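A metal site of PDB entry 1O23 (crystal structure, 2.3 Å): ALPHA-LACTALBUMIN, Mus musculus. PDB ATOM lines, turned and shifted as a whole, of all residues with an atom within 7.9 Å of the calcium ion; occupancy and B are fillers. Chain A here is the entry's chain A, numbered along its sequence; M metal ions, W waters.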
ATOM      1  N   THR A  38     -35.208  19.908 -25.213  1.00  0.00           N
ATOM      2  CA  THR A  38     -33.964  20.030 -24.444  1.00  0.00           C
ATOM      3  C   THR A  38     -34.165  20.119 -22.932  1.00  0.00           C
ATOM      4  O   THR A  38     -33.194  19.947 -22.178  1.00  0.00           O
ATOM      5  CB  THR A  38     -33.176  21.293 -24.854  1.00  0.00           C
ATOM      6  OG1 THR A  38     -33.947  22.469 -24.530  1.00  0.00           O
ATOM      7  CG2 THR A  38     -32.863  21.289 -26.349  1.00  0.00           C
ATOM      8  N   ILE A  75     -20.475  15.800 -15.278  1.00  0.00           N
ATOM      9  CA  ILE A  75     -21.224  17.033 -15.469  1.00  0.00           C
ATOM     10  C   ILE A  75     -22.457  17.038 -14.594  1.00  0.00           C
ATOM     11  O   ILE A  75     -23.010  15.984 -14.244  1.00  0.00           O
ATOM     12  CB  ILE A  75     -21.734  17.189 -16.949  1.00  0.00           C
ATOM     13  CG1 ILE A  75     -22.668  16.030 -17.294  1.00  0.00           C
ATOM     14  CG2 ILE A  75     -20.558  17.259 -17.915  1.00  0.00           C
ATOM     15  CD1 ILE A  75     -23.170  16.061 -18.715  1.00  0.00           C
ATOM     16  N   SER A  76     -22.896  18.233 -14.245  1.00  0.00           N
ATOM     17  CA  SER A  76     -24.105  18.329 -13.450  1.00  0.00           C
ATOM     18  C   SER A  76     -25.240  18.036 -14.429  1.00  0.00           C
ATOM     19  O   SER A  76     -25.240  18.536 -15.547  1.00  0.00           O
ATOM     20  CB  SER A  76     -24.250  19.747 -12.885  1.00  0.00           C
ATOM     21  OG  SER A  76     -25.493  19.863 -12.218  1.00  0.00           O
ATOM     22  N   CYS A  77     -26.205  17.229 -14.020  1.00  0.00           N
ATOM     23  CA  CYS A  77     -27.342  16.908 -14.878  1.00  0.00           C
ATOM     24  C   CYS A  77     -28.085  18.178 -15.384  1.00  0.00           C
ATOM     25  O   CYS A  77     -28.622  18.181 -16.511  1.00  0.00           O
ATOM     26  CB  CYS A  77     -28.318  15.997 -14.115  1.00  0.00           C
ATOM     27  SG  CYS A  77     -27.709  14.335 -13.594  1.00  0.00           S
ATOM     28  N   ASP A  78     -28.094  19.239 -14.574  1.00  0.00           N
ATOM     29  CA  ASP A  78     -28.782  20.501 -14.929  1.00  0.00           C
ATOM     30  C   ASP A  78     -28.172  21.129 -16.144  1.00  0.00           C
ATOM     31  O   ASP A  78     -28.795  21.952 -16.810  1.00  0.00           O
ATOM     32  CB  ASP A  78     -28.730  21.540 -13.797  1.00  0.00           C
ATOM     33  CG  ASP A  78     -29.353  21.051 -12.513  1.00  0.00           C
ATOM     34  OD1 ASP A  78     -30.364  20.309 -12.573  1.00  0.00           O
ATOM     35  OD2 ASP A  78     -28.838  21.417 -11.438  1.00  0.00           O
ATOM     36  N   LYS A  79     -26.928  20.760 -16.438  1.00  0.00           N
ATOM     37  CA  LYS A  79     -26.270  21.299 -17.612  1.00  0.00           C
ATOM     38  C   LYS A  79     -26.844  20.674 -18.891  1.00  0.00           C
ATOM     39  O   LYS A  79     -26.506  21.091 -19.999  1.00  0.00           O
ATOM     40  CB  LYS A  79     -24.769  21.051 -17.529  1.00  0.00           C
ATOM     41  CG  LYS A  79     -23.974  22.230 -16.984  1.00  0.00           C
ATOM     42  CD  LYS A  79     -24.515  22.728 -15.645  1.00  0.00           C
ATOM     43  CE  LYS A  79     -24.094  24.179 -15.356  1.00  0.00           C
ATOM     44  NZ  LYS A  79     -24.841  25.152 -16.201  1.00  0.00           N
ATOM     45  N   LEU A  80     -27.690  19.663 -18.713  1.00  0.00           N
ATOM     46  CA  LEU A  80     -28.312  18.977 -19.841  1.00  0.00           C
ATOM     47  C   LEU A  80     -29.721  19.517 -20.055  1.00  0.00           C
ATOM     48  O   LEU A  80     -30.485  19.002 -20.887  1.00  0.00           O
ATOM     49  CB  LEU A  80     -28.362  17.464 -19.590  1.00  0.00           C
ATOM     50  CG  LEU A  80     -27.000  16.795 -19.381  1.00  0.00           C
ATOM     51  CD1 LEU A  80     -27.164  15.433 -18.724  1.00  0.00           C
ATOM     52  CD2 LEU A  80     -26.297  16.690 -20.714  1.00  0.00           C
ATOM     53  N   LEU A  81     -30.063  20.566 -19.302  1.00  0.00           N
ATOM     54  CA  LEU A  81     -31.376  21.170 -19.417  1.00  0.00           C
ATOM     55  C   LEU A  81     -31.334  22.568 -20.010  1.00  0.00           C
ATOM     56  O   LEU A  81     -32.349  23.264 -20.008  1.00  0.00           O
ATOM     57  CB  LEU A  81     -32.065  21.236 -18.065  1.00  0.00           C
ATOM     58  CG  LEU A  81     -32.357  19.906 -17.385  1.00  0.00           C
ATOM     59  CD1 LEU A  81     -32.985  20.207 -16.052  1.00  0.00           C
ATOM     60  CD2 LEU A  81     -33.277  19.028 -18.217  1.00  0.00           C
ATOM     61  N   ASP A  82     -30.163  23.002 -20.478  1.00  0.00           N
ATOM     62  CA  ASP A  82     -30.106  24.315 -21.092  1.00  0.00           C
ATOM     63  C   ASP A  82     -30.213  24.079 -22.584  1.00  0.00           C
ATOM     64  O   ASP A  82     -30.648  23.010 -22.994  1.00  0.00           O
ATOM     65  CB  ASP A  82     -28.813  25.078 -20.731  1.00  0.00           C
ATOM     66  CG  ASP A  82     -27.545  24.345 -21.114  1.00  0.00           C
ATOM     67  OD1 ASP A  82     -27.463  23.782 -22.224  1.00  0.00           O
ATOM     68  OD2 ASP A  82     -26.605  24.362 -20.298  1.00  0.00           O
ATOM     69  N   ASP A  83     -29.859  25.059 -23.400  1.00  0.00           N
ATOM     70  CA  ASP A  83     -29.953  24.858 -24.837  1.00  0.00           C
ATOM     71  C   ASP A  83     -28.616  24.742 -25.538  1.00  0.00           C
ATOM     72  O   ASP A  83     -28.539  24.884 -26.753  1.00  0.00           O
ATOM     73  CB  ASP A  83     -30.803  25.951 -25.471  1.00  0.00           C
ATOM     74  CG  ASP A  83     -32.308  25.784 -25.178  1.00  0.00           C
ATOM     75  OD1 ASP A  83     -32.653  25.233 -24.109  1.00  0.00           O
ATOM     76  OD2 ASP A  83     -33.139  26.211 -26.003  1.00  0.00           O
ATOM     77  N   GLU A  84     -27.557  24.496 -24.757  1.00  0.00           N
ATOM     78  CA  GLU A  84     -26.223  24.294 -25.322  1.00  0.00           C
ATOM     79  C   GLU A  84     -26.016  22.770 -25.304  1.00  0.00           C
ATOM     80  O   GLU A  84     -25.872  22.152 -24.251  1.00  0.00           O
ATOM     81  CB  GLU A  84     -25.145  25.037 -24.517  1.00  0.00           C
ATOM     82  CG  GLU A  84     -24.953  26.487 -24.977  1.00  0.00           C
ATOM     83  CD  GLU A  84     -23.763  27.216 -24.330  1.00  0.00           C
ATOM     84  OE1 GLU A  84     -22.822  26.555 -23.838  1.00  0.00           O
ATOM     85  OE2 GLU A  84     -23.758  28.465 -24.332  1.00  0.00           O
ATOM     86  N   LEU A  85     -26.030  22.185 -26.494  1.00  0.00           N
ATOM     87  CA  LEU A  85     -25.915  20.746 -26.694  1.00  0.00           C
ATOM     88  C   LEU A  85     -24.511  20.115 -26.675  1.00  0.00           C
ATOM     89  O   LEU A  85     -24.377  18.883 -26.706  1.00  0.00           O
ATOM     90  CB  LEU A  85     -26.634  20.370 -28.003  1.00  0.00           C
ATOM     91  CG  LEU A  85     -28.102  19.966 -27.834  1.00  0.00           C
ATOM     92  CD1 LEU A  85     -28.724  20.835 -26.771  1.00  0.00           C
ATOM     93  CD2 LEU A  85     -28.887  20.043 -29.195  1.00  0.00           C
ATOM     94  N   ASP A  86     -23.478  20.946 -26.609  1.00  0.00           N
ATOM     95  CA  ASP A  86     -22.117  20.436 -26.626  1.00  0.00           C
ATOM     96  C   ASP A  86     -21.842  19.387 -25.557  1.00  0.00           C
ATOM     97  O   ASP A  86     -21.352  18.294 -25.858  1.00  0.00           O
ATOM     98  CB  ASP A  86     -21.135  21.606 -26.535  1.00  0.00           C
ATOM     99  CG  ASP A  86     -21.338  22.623 -27.660  1.00  0.00           C
ATOM    100  OD1 ASP A  86     -22.295  23.458 -27.540  1.00  0.00           O
ATOM    101  OD2 ASP A  86     -20.583  22.588 -28.664  1.00  0.00           O
ATOM    102  N   ASP A  87     -22.180  19.690 -24.310  1.00  0.00           N
ATOM    103  CA  ASP A  87     -21.929  18.721 -23.271  1.00  0.00           C
ATOM    104  C   ASP A  87     -22.872  17.511 -23.331  1.00  0.00           C
ATOM    105  O   ASP A  87     -22.477  16.401 -22.976  1.00  0.00           O
ATOM    106  CB  ASP A  87     -21.970  19.391 -21.874  1.00  0.00           C
ATOM    107  CG  ASP A  87     -23.175  20.323 -21.669  1.00  0.00           C
ATOM    108  OD1 ASP A  87     -24.093  20.350 -22.528  1.00  0.00           O
ATOM    109  OD2 ASP A  87     -23.191  21.026 -20.626  1.00  0.00           O
ATOM    110  N   ASP A  88     -24.109  17.722 -23.797  1.00  0.00           N
ATOM    111  CA  ASP A  88     -25.064  16.627 -23.926  1.00  0.00           C
ATOM    112  C   ASP A  88     -24.454  15.664 -24.934  1.00  0.00           C
ATOM    113  O   ASP A  88     -24.406  14.455 -24.710  1.00  0.00           O
ATOM    114  CB  ASP A  88     -26.427  17.101 -24.461  1.00  0.00           C
ATOM    115  CG  ASP A  88     -27.051  18.199 -23.619  1.00  0.00           C
ATOM    116  OD1 ASP A  88     -28.193  18.064 -23.163  1.00  0.00           O
ATOM    117  OD2 ASP A  88     -26.405  19.232 -23.413  1.00  0.00           O
ATOM    118  N   ILE A  89     -23.961  16.202 -26.035  1.00  0.00           N
ATOM    119  CA  ILE A  89     -23.373  15.381 -27.057  1.00  0.00           C
ATOM    120  C   ILE A  89     -22.149  14.605 -26.607  1.00  0.00           C
ATOM    121  O   ILE A  89     -22.037  13.403 -26.856  1.00  0.00           O
ATOM    122  CB  ILE A  89     -23.039  16.220 -28.271  1.00  0.00           C
ATOM    123  CG1 ILE A  89     -24.346  16.809 -28.836  1.00  0.00           C
ATOM    124  CG2 ILE A  89     -22.281  15.374 -29.322  1.00  0.00           C
ATOM    125  CD1 ILE A  89     -24.151  17.816 -29.981  1.00  0.00           C
HETATM  126 CA    CA M   1     -26.127  21.375 -22.279  1.00  0.00          CA
HETATM  127  O   HOH W   1     -28.759  21.062 -22.220  1.00  0.00           O
HETATM  128  O   HOH W   2     -24.511  23.104 -21.108  1.00  0.00           O
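Water W2 lies within hydrogen-bond range of the side-chain carboxylate (OD2) of Asp 87 (2.5 Å) and the side-chain carboxylate (OD2) of Asp 82 (2.6 Å).
Five residues have an atom within 4 Å of the calcium ion: Lys 79, Asp 82, Glu 84, Asp 87 and Asp 88.
The calcium ion is bound by O of Glu 84 (2.1 Å), OD1 of Asp 87 (2.3 Å), O of Lys 79 (2.3 Å), OD2 of Asp 88 (2.4 Å), water W2 (2.6 Å), water W1 (2.7 Å) and OD1 of Asp 82 (2.8 Å).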
